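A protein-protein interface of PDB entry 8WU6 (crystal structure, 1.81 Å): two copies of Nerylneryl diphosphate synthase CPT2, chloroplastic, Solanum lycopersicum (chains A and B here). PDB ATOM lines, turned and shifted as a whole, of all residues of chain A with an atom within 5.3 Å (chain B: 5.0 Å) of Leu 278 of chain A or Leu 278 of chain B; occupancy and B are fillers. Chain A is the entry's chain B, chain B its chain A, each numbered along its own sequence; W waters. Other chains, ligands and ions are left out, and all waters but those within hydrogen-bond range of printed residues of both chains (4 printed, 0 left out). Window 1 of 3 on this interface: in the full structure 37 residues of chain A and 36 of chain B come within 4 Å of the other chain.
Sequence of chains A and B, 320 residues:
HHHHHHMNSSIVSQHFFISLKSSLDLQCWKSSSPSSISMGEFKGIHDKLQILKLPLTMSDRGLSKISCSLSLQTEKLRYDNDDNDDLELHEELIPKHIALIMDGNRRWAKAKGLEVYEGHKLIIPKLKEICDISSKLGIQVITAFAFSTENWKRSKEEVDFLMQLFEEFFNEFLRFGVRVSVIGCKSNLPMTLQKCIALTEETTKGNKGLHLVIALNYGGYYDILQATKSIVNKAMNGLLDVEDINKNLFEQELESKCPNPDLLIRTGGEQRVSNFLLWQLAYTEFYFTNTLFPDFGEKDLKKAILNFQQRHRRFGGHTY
N of Asn 275 of chain B lies within hydrogen-bond range of O of Ala 282 of chain A.
The backbone carbonyl oxygen (O) of Ala 282 of chain B is in hydrogen-bond range of the backbone NH (N) of Asn 275 of chain A (2.9 Å).
The backbone carbonyl oxygen of Asn 275 of chain B lies within hydrogen-bond range of the backbone NH of Gly 220 of chain B (2.8 Å).
N of Tyr 221 of chain B lies within hydrogen-bond range of OD1 of Asn 275 of chain B (3.0 Å).
The backbone carbonyl oxygen (O) of Asn 275 of chain A lies within hydrogen-bond range of the backbone NH (N) of Gly 220 of chain A, 2.9 Å away.
The backbone NH (N) of Tyr 221 of chain A is in hydrogen-bond range of the side-chain amide oxygen (OD1) of Asn 275 of chain A.
Ala 282 of chain B touches Tyr 221 of chain A (CB to OH, 3.5 Å).
CD1 of Ile 224 of chain B touches CD1 of Ile 224 of chain A, 3.9 Å away.
Ile 224 of chain A touches Trp 279 of chain B (CG2 to CZ3, 3.7 Å).
Leu 281 of chain B touches Val 273 of chain A.
O of Ala 282 of chain B touches CG2 of Val 273 of chain A (3.7 Å).
Leu 278 of chain A touches Leu 278 of chain B (O to CD2, 3.7 Å).
CZ2 of Trp 279 of chain A touches CD1 of Tyr 221 of chain B (3.5 Å).
CG2 of Ile 224 of chain B touches CZ3 of Trp 279 of chain A (3.8 Å).
Leu 281 of chain A touches Val 273 of chain B.
Ala 282 of chain A touches Leu 278 of chain B.
Of the printed residues of chain B, Asn 275 of chain A touches Ala 282 (2.9 Å).
Leu 278 of chain A touches just these residues of chain B: Leu 278 (3.7 Å) and Ala 282 (3.7 Å).
Printed residues of chain B within 4 Å of Ala 282 of chain A: Tyr 221 (3.4 Å), Val 273 (3.8 Å), Asn 275 (2.9 Å) and Leu 278 (3.7 Å).
Leu 278 of chain B touches just these residues of chain A: Leu 278 and Ala 282.
Printed residues of chain A within 4 Å of Trp 279 of chain B: Tyr 221 and Ile 224.
The nearest residue of chain B that does not touch Leu 278 of chain A is Trp 279 of chain B (4.1 Å).
The nearest residue of chain A that does not touch Leu 278 of chain B is Trp 279 of chain A (4.04 Å).
Printed residues of chain A that touch a printed residue of chain B: Tyr 221, Ile 224, Val 273, Asn 275, Leu 278, Trp 279, Leu 281 and Ala 282.
Hydrophobic or aromatic side chains of chain A within 4 Å of the printed part of chain B: Tyr 221, Ile 224, Val 273, Leu 278, Trp 279 and Ala 282.
Of the 12 printed residues of chain B, 8 touch a printed residue of chain A.
Printed residues of chain B that touch a printed residue of chain A: Tyr 221, Ile 224, Val 273, Asn 275, Leu 278, Trp 279, Leu 281 and Ala 282.
Among the printed residues, 16 pairs touch across the chains.
Tyr 221 of chain A touches Trp 279 of chain B, and with the chains exchanged Trp 279 of chain A touches Tyr 221 of chain B.
Tyr 221 of chain A touches Ala 282 of chain B, and with the chains exchanged Ala 282 of chain A touches Tyr 221 of chain B.
Ile 224 of chain B touches its own counterpart, Ile 224 of chain A.
Leu 278 of chain A touches Ala 282 of chain B, and with the chains exchanged Ala 282 of chain A touches Leu 278 of chain B.
12 positions are printed for both chains.
Of the 16 pairs that touch across the chains among the printed residues, 16 have their exchanged pair printed and touching as well.
Water W2 lies within hydrogen-bond range of the side-chain hydroxyl (OH) of Tyr 221 of chain A (2.7 Å) and the backbone carbonyl oxygen (O) of Trp 279 of chain B (2.7 Å).
Water W4 lies within hydrogen-bond range of the backbone carbonyl oxygen of Trp 279 of chain A (2.7 Å), the side-chain hydroxyl of Tyr 221 of chain B (2.7 Å) and the backbone carbonyl oxygen of Gln 280 of chain A (3.5 Å).
Water W3 lies within hydrogen-bond range of N of Val 273 of chain B, O of Leu 281 of chain A and O of Ala 282 of chain A.
Water W1 lies within hydrogen-bond range of the backbone NH (N) of Val 273 of chain A, the backbone carbonyl oxygen (O) of Leu 281 of chain B and the backbone carbonyl oxygen (O) of Ala 282 of chain B.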
ATOM      1  N   GLY A 220      -2.017  10.909   2.807  1.00  0.00           N
ATOM      2  CA  GLY A 220      -3.047   9.874   2.814  1.00  0.00           C
ATOM      3  C   GLY A 220      -3.851   9.872   4.104  1.00  0.00           C
ATOM      4  O   GLY A 220      -5.075   9.703   4.083  1.00  0.00           O
ATOM      5  N   TYR A 221      -3.167  10.014   5.242  1.00  0.00           N
ATOM      6  CA  TYR A 221      -3.880  10.160   6.516  1.00  0.00           C
ATOM      7  C   TYR A 221      -4.826  11.353   6.477  1.00  0.00           C
ATOM      8  O   TYR A 221      -5.993  11.255   6.887  1.00  0.00           O
ATOM      9  CB  TYR A 221      -2.917  10.366   7.680  1.00  0.00           C
ATOM     10  CG  TYR A 221      -1.896   9.275   7.970  1.00  0.00           C
ATOM     11  CD1 TYR A 221      -2.190   7.922   7.830  1.00  0.00           C
ATOM     12  CD2 TYR A 221      -0.658   9.637   8.475  1.00  0.00           C
ATOM     13  CE1 TYR A 221      -1.204   6.929   8.161  1.00  0.00           C
ATOM     14  CE2 TYR A 221       0.306   8.688   8.800  1.00  0.00           C
ATOM     15  CZ  TYR A 221       0.031   7.353   8.649  1.00  0.00           C
ATOM     16  OH  TYR A 221       1.055   6.478   9.002  1.00  0.00           O
ATOM     17  N   ILE A 224      -8.095  10.669   4.415  1.00  0.00           N
ATOM     18  CA  ILE A 224      -9.024   9.775   5.118  1.00  0.00           C
ATOM     19  C   ILE A 224      -9.651  10.476   6.326  1.00  0.00           C
ATOM     20  O   ILE A 224     -10.856  10.330   6.597  1.00  0.00           O
ATOM     21  CB  ILE A 224      -8.281   8.484   5.505  1.00  0.00           C
ATOM     22  CG1 ILE A 224      -8.077   7.631   4.243  1.00  0.00           C
ATOM     23  CG2 ILE A 224      -9.089   7.683   6.550  1.00  0.00           C
ATOM     24  CD1 ILE A 224      -6.943   6.613   4.379  1.00  0.00           C
ATOM     25  N   VAL A 273       5.634   4.431  -0.134  1.00  0.00           N
ATOM     26  CA  VAL A 273       4.724   5.456  -0.649  1.00  0.00           C
ATOM     27  C   VAL A 273       4.702   6.720   0.223  1.00  0.00           C
ATOM     28  O   VAL A 273       4.140   7.746  -0.208  1.00  0.00           O
ATOM     29  CB  VAL A 273       3.297   4.891  -0.830  1.00  0.00           C
ATOM     30  CG1 VAL A 273       3.302   3.667  -1.775  1.00  0.00           C
ATOM     31  CG2 VAL A 273       2.684   4.505   0.503  1.00  0.00           C
ATOM     32  N   ASN A 275       3.123   8.001   2.751  1.00  0.00           N
ATOM     33  CA  ASN A 275       1.864   8.693   3.120  1.00  0.00           C
ATOM     34  C   ASN A 275       1.329   9.594   1.994  1.00  0.00           C
ATOM     35  O   ASN A 275       0.848  10.700   2.235  1.00  0.00           O
ATOM     36  CB  ASN A 275       2.057   9.506   4.412  1.00  0.00           C
ATOM     37  CG  ASN A 275       0.746  10.061   4.956  1.00  0.00           C
ATOM     38  OD1 ASN A 275      -0.305   9.456   4.778  1.00  0.00           O
ATOM     39  ND2 ASN A 275       0.802  11.265   5.554  1.00  0.00           N
ATOM     40  N   PHE A 276       1.437   9.128   0.750  1.00  0.00           N
ATOM     41  CA  PHE A 276       0.796   9.726  -0.423  1.00  0.00           C
ATOM     42  C   PHE A 276      -0.636   9.171  -0.433  1.00  0.00           C
ATOM     43  O   PHE A 276      -1.286   9.135   0.624  1.00  0.00           O
ATOM     44  CB  PHE A 276       1.631   9.403  -1.697  1.00  0.00           C
ATOM     45  CG  PHE A 276       1.274  10.209  -2.949  1.00  0.00           C
ATOM     46  CD1 PHE A 276       0.604  11.424  -2.887  1.00  0.00           C
ATOM     47  CD2 PHE A 276       1.637   9.725  -4.210  1.00  0.00           C
ATOM     48  CE1 PHE A 276       0.301  12.125  -4.051  1.00  0.00           C
ATOM     49  CE2 PHE A 276       1.356  10.431  -5.374  1.00  0.00           C
ATOM     50  CZ  PHE A 276       0.684  11.639  -5.295  1.00  0.00           C
ATOM     51  N   LEU A 277      -1.131   8.656  -1.543  1.00  0.00           N
ATOM     52  CA  LEU A 277      -2.562   8.372  -1.747  1.00  0.00           C
ATOM     53  C   LEU A 277      -3.061   7.002  -1.232  1.00  0.00           C
ATOM     54  O   LEU A 277      -3.455   6.135  -2.027  1.00  0.00           O
ATOM     55  CB  LEU A 277      -2.847   8.436  -3.233  1.00  0.00           C
ATOM     56  CG  LEU A 277      -2.563   9.702  -3.992  1.00  0.00           C
ATOM     57  CD1 LEU A 277      -2.479   9.358  -5.475  1.00  0.00           C
ATOM     58  CD2 LEU A 277      -3.680  10.676  -3.695  1.00  0.00           C
ATOM     59  N   LEU A 278      -3.198   6.856   0.090  1.00  0.00           N
ATOM     60  CA  LEU A 278      -3.333   5.520   0.702  1.00  0.00           C
ATOM     61  C   LEU A 278      -4.570   4.754   0.215  1.00  0.00           C
ATOM     62  O   LEU A 278      -4.459   3.631  -0.296  1.00  0.00           O
ATOM     63  CB  LEU A 278      -3.348   5.650   2.227  1.00  0.00           C
ATOM     64  CG  LEU A 278      -2.068   6.263   2.779  1.00  0.00           C
ATOM     65  CD1 LEU A 278      -2.199   6.452   4.287  1.00  0.00           C
ATOM     66  CD2 LEU A 278      -0.848   5.378   2.427  1.00  0.00           C
ATOM     67  N   TRP A 279      -5.767   5.325   0.404  1.00  0.00           N
ATOM     68  CA  TRP A 279      -6.987   4.650  -0.027  1.00  0.00           C
ATOM     69  C   TRP A 279      -6.955   4.385  -1.533  1.00  0.00           C
ATOM     70  O   TRP A 279      -7.354   3.314  -2.012  1.00  0.00           O
ATOM     71  CB  TRP A 279      -8.194   5.534   0.333  1.00  0.00           C
ATOM     72  CG  TRP A 279      -9.543   5.059  -0.254  1.00  0.00           C
ATOM     73  CD1 TRP A 279      -9.980   5.185  -1.547  1.00  0.00           C
ATOM     74  CD2 TRP A 279     -10.606   4.404   0.466  1.00  0.00           C
ATOM     75  NE1 TRP A 279     -11.253   4.633  -1.678  1.00  0.00           N
ATOM     76  CE2 TRP A 279     -11.657   4.171  -0.449  1.00  0.00           C
ATOM     77  CE3 TRP A 279     -10.770   3.995   1.807  1.00  0.00           C
ATOM     78  CZ2 TRP A 279     -12.856   3.548  -0.072  1.00  0.00           C
ATOM     79  CZ3 TRP A 279     -11.971   3.381   2.171  1.00  0.00           C
ATOM     80  CH2 TRP A 279     -12.991   3.167   1.233  1.00  0.00           C
ATOM     81  N   GLN A 280      -6.454   5.346  -2.286  1.00  0.00           N
ATOM     82  CA  GLN A 280      -6.530   5.328  -3.731  1.00  0.00           C
ATOM     83  C   GLN A 280      -5.515   4.370  -4.358  1.00  0.00           C
ATOM     84  O   GLN A 280      -5.599   4.132  -5.562  1.00  0.00           O
ATOM     85  CB  GLN A 280      -6.316   6.762  -4.257  1.00  0.00           C
ATOM     86  CG  GLN A 280      -7.458   7.763  -3.838  1.00  0.00           C
ATOM     87  CD  GLN A 280      -7.229   8.424  -2.481  1.00  0.00           C
ATOM     88  OE1 GLN A 280      -6.315   8.074  -1.731  1.00  0.00           O
ATOM     89  NE2 GLN A 280      -8.114   9.356  -2.133  1.00  0.00           N
ATOM     90  N   LEU A 281      -4.578   3.812  -3.582  1.00  0.00           N
ATOM     91  CA  LEU A 281      -3.528   2.947  -4.133  1.00  0.00           C
ATOM     92  C   LEU A 281      -3.813   1.457  -3.962  1.00  0.00           C
ATOM     93  O   LEU A 281      -2.901   0.613  -4.170  1.00  0.00           O
ATOM     94  CB  LEU A 281      -2.184   3.292  -3.486  1.00  0.00           C
ATOM     95  CG  LEU A 281      -1.632   4.667  -3.853  1.00  0.00           C
ATOM     96  CD1 LEU A 281      -0.320   4.964  -3.043  1.00  0.00           C
ATOM     97  CD2 LEU A 281      -1.412   4.843  -5.338  1.00  0.00           C
ATOM     98  N   ALA A 282      -5.054   1.102  -3.638  1.00  0.00           N
ATOM     99  CA  ALA A 282      -5.378  -0.270  -3.268  1.00  0.00           C
ATOM    100  C   ALA A 282      -5.018  -1.272  -4.361  1.00  0.00           C
ATOM    101  O   ALA A 282      -4.657  -2.420  -4.062  1.00  0.00           O
ATOM    102  CB  ALA A 282      -6.871  -0.362  -2.910  1.00  0.00           C
ATOM    103  N   GLY B 220      -8.466  -3.442   3.048  1.00  0.00           N
ATOM    104  CA  GLY B 220      -8.162  -2.095   3.538  1.00  0.00           C
ATOM    105  C   GLY B 220      -9.373  -1.169   3.545  1.00  0.00           C
ATOM    106  O   GLY B 220      -9.560  -0.384   4.485  1.00  0.00           O
ATOM    107  N   TYR B 221     -10.177  -1.200   2.475  1.00  0.00           N
ATOM    108  CA  TYR B 221     -11.420  -0.420   2.456  1.00  0.00           C
ATOM    109  C   TYR B 221     -12.301  -0.772   3.635  1.00  0.00           C
ATOM    110  O   TYR B 221     -12.857   0.120   4.298  1.00  0.00           O
ATOM    111  CB  TYR B 221     -12.219  -0.695   1.190  1.00  0.00           C
ATOM    112  CG  TYR B 221     -11.570  -0.402  -0.126  1.00  0.00           C
ATOM    113  CD1 TYR B 221     -10.774   0.728  -0.321  1.00  0.00           C
ATOM    114  CD2 TYR B 221     -11.830  -1.233  -1.207  1.00  0.00           C
ATOM    115  CE1 TYR B 221     -10.223   0.999  -1.598  1.00  0.00           C
ATOM    116  CE2 TYR B 221     -11.281  -0.984  -2.453  1.00  0.00           C
ATOM    117  CZ  TYR B 221     -10.496   0.129  -2.643  1.00  0.00           C
ATOM    118  OH  TYR B 221     -10.004   0.340  -3.918  1.00  0.00           O
ATOM    119  N   ILE B 224     -10.966   0.690   7.011  1.00  0.00           N
ATOM    120  CA  ILE B 224     -11.193   2.132   7.098  1.00  0.00           C
ATOM    121  C   ILE B 224     -12.683   2.445   7.272  1.00  0.00           C
ATOM    122  O   ILE B 224     -13.053   3.311   8.063  1.00  0.00           O
ATOM    123  CB  ILE B 224     -10.582   2.823   5.863  1.00  0.00           C
ATOM    124  CG1 ILE B 224      -9.043   2.797   5.955  1.00  0.00           C
ATOM    125  CG2 ILE B 224     -11.132   4.285   5.751  1.00  0.00           C
ATOM    126  CD1 ILE B 224      -8.341   3.009   4.605  1.00  0.00           C
ATOM    127  N   VAL B 273      -0.509  -3.936  -3.719  1.00  0.00           N
ATOM    128  CA  VAL B 273      -0.880  -4.361  -2.367  1.00  0.00           C
ATOM    129  C   VAL B 273      -2.270  -4.981  -2.313  1.00  0.00           C
ATOM    130  O   VAL B 273      -2.627  -5.589  -1.280  1.00  0.00           O
ATOM    131  CB  VAL B 273      -0.746  -3.202  -1.356  1.00  0.00           C
ATOM    132  CG1 VAL B 273       0.715  -2.740  -1.295  1.00  0.00           C
ATOM    133  CG2 VAL B 273      -1.713  -2.052  -1.672  1.00  0.00           C
ATOM    134  N   ASN B 275      -5.440  -4.190  -1.945  1.00  0.00           N
ATOM    135  CA  ASN B 275      -6.428  -3.863  -0.901  1.00  0.00           C
ATOM    136  C   ASN B 275      -6.162  -4.600   0.421  1.00  0.00           C
ATOM    137  O   ASN B 275      -7.090  -5.012   1.115  1.00  0.00           O
ATOM    138  CB  ASN B 275      -7.850  -4.136  -1.419  1.00  0.00           C
ATOM    139  CG  ASN B 275      -8.930  -3.588  -0.482  1.00  0.00           C
ATOM    140  OD1 ASN B 275      -8.733  -2.567   0.177  1.00  0.00           O
ATOM    141  ND2 ASN B 275     -10.053  -4.303  -0.394  1.00  0.00           N
ATOM    142  N   PHE B 276      -4.881  -4.739   0.792  1.00  0.00           N
ATOM    143  CA  PHE B 276      -4.456  -5.240   2.107  1.00  0.00           C
ATOM    144  C   PHE B 276      -4.484  -4.065   3.104  1.00  0.00           C
ATOM    145  O   PHE B 276      -5.462  -3.313   3.113  1.00  0.00           O
ATOM    146  CB  PHE B 276      -3.069  -5.930   1.934  1.00  0.00           C
ATOM    147  CG  PHE B 276      -2.606  -6.787   3.100  1.00  0.00           C
ATOM    148  CD1 PHE B 276      -3.483  -7.283   4.043  1.00  0.00           C
ATOM    149  CD2 PHE B 276      -1.254  -7.108   3.224  1.00  0.00           C
ATOM    150  CE1 PHE B 276      -3.004  -8.053   5.115  1.00  0.00           C
ATOM    151  CE2 PHE B 276      -0.778  -7.897   4.276  1.00  0.00           C
ATOM    152  CZ  PHE B 276      -1.650  -8.370   5.201  1.00  0.00           C
ATOM    153  N   LEU B 277      -3.435  -3.820   3.886  1.00  0.00           N
ATOM    154  CA  LEU B 277      -3.451  -2.882   5.027  1.00  0.00           C
ATOM    155  C   LEU B 277      -3.196  -1.409   4.648  1.00  0.00           C
ATOM    156  O   LEU B 277      -2.179  -0.823   5.029  1.00  0.00           O
ATOM    157  CB  LEU B 277      -2.386  -3.311   6.022  1.00  0.00           C
ATOM    158  CG  LEU B 277      -2.372  -4.754   6.470  1.00  0.00           C
ATOM    159  CD1 LEU B 277      -1.117  -4.954   7.295  1.00  0.00           C
ATOM    160  CD2 LEU B 277      -3.609  -5.004   7.324  1.00  0.00           C
ATOM    161  N   LEU B 278      -4.172  -0.776   3.985  1.00  0.00           N
ATOM    162  CA  LEU B 278      -3.931   0.486   3.268  1.00  0.00           C
ATOM    163  C   LEU B 278      -3.407   1.592   4.186  1.00  0.00           C
ATOM    164  O   LEU B 278      -2.342   2.180   3.933  1.00  0.00           O
ATOM    165  CB  LEU B 278      -5.214   0.933   2.560  1.00  0.00           C
ATOM    166  CG  LEU B 278      -5.691   0.009   1.442  1.00  0.00           C
ATOM    167  CD1 LEU B 278      -7.005   0.522   0.884  1.00  0.00           C
ATOM    168  CD2 LEU B 278      -4.640  -0.042   0.340  1.00  0.00           C
ATOM    169  N   TRP B 279      -4.151   1.909   5.255  1.00  0.00           N
ATOM    170  CA  TRP B 279      -3.708   2.961   6.169  1.00  0.00           C
ATOM    171  C   TRP B 279      -2.371   2.595   6.795  1.00  0.00           C
ATOM    172  O   TRP B 279      -1.476   3.448   6.935  1.00  0.00           O
ATOM    173  CB  TRP B 279      -4.772   3.168   7.265  1.00  0.00           C
ATOM    174  CG  TRP B 279      -4.361   4.070   8.422  1.00  0.00           C
ATOM    175  CD1 TRP B 279      -3.489   3.774   9.436  1.00  0.00           C
ATOM    176  CD2 TRP B 279      -4.860   5.389   8.692  1.00  0.00           C
ATOM    177  NE1 TRP B 279      -3.389   4.846  10.312  1.00  0.00           N
ATOM    178  CE2 TRP B 279      -4.210   5.854   9.862  1.00  0.00           C
ATOM    179  CE3 TRP B 279      -5.763   6.238   8.035  1.00  0.00           C
ATOM    180  CZ2 TRP B 279      -4.466   7.110  10.417  1.00  0.00           C
ATOM    181  CZ3 TRP B 279      -6.003   7.498   8.578  1.00  0.00           C
ATOM    182  CH2 TRP B 279      -5.352   7.925   9.760  1.00  0.00           C
ATOM    183  N   GLN B 280      -2.214   1.321   7.156  1.00  0.00           N
ATOM    184  CA  GLN B 280      -1.073   0.876   7.946  1.00  0.00           C
ATOM    185  C   GLN B 280       0.208   0.766   7.123  1.00  0.00           C
ATOM    186  O   GLN B 280       1.291   0.634   7.708  1.00  0.00           O
ATOM    187  CB  GLN B 280      -1.400  -0.475   8.585  1.00  0.00           C
ATOM    188  CG  GLN B 280      -2.605  -0.410   9.572  1.00  0.00           C
ATOM    189  CD  GLN B 280      -3.973  -0.629   8.930  1.00  0.00           C
ATOM    190  OE1 GLN B 280      -4.150  -0.593   7.693  1.00  0.00           O
ATOM    191  NE2 GLN B 280      -4.976  -0.845   9.792  1.00  0.00           N
ATOM    192  N   LEU B 281       0.128   0.870   5.798  1.00  0.00           N
ATOM    193  CA  LEU B 281       1.307   0.729   4.936  1.00  0.00           C
ATOM    194  C   LEU B 281       1.923   2.076   4.533  1.00  0.00           C
ATOM    195  O   LEU B 281       2.774   2.126   3.622  1.00  0.00           O
ATOM    196  CB  LEU B 281       0.923  -0.059   3.672  1.00  0.00           C
ATOM    197  CG  LEU B 281       0.624  -1.561   3.913  1.00  0.00           C
ATOM    198  CD1 LEU B 281       0.061  -2.224   2.637  1.00  0.00           C
ATOM    199  CD2 LEU B 281       1.849  -2.337   4.422  1.00  0.00           C
ATOM    200  N   ALA B 282       1.533   3.171   5.192  1.00  0.00           N
ATOM    201  CA  ALA B 282       1.939   4.508   4.743  1.00  0.00           C
ATOM    202  C   ALA B 282       3.458   4.696   4.677  1.00  0.00           C
ATOM    203  O   ALA B 282       3.942   5.485   3.856  1.00  0.00           O
ATOM    204  CB  ALA B 282       1.323   5.571   5.672  1.00  0.00           C
HETATM  205  O   HOH W   1       5.182   2.924   2.242  1.00  0.00           O
HETATM  206  O   HOH W   2       0.489   3.897   8.755  1.00  0.00           O
HETATM  207  O   HOH W   3      -1.620  -1.730  -5.081  1.00  0.00           O
HETATM  208  O   HOH W   4      -8.356   2.431  -4.349  1.00  0.00           O
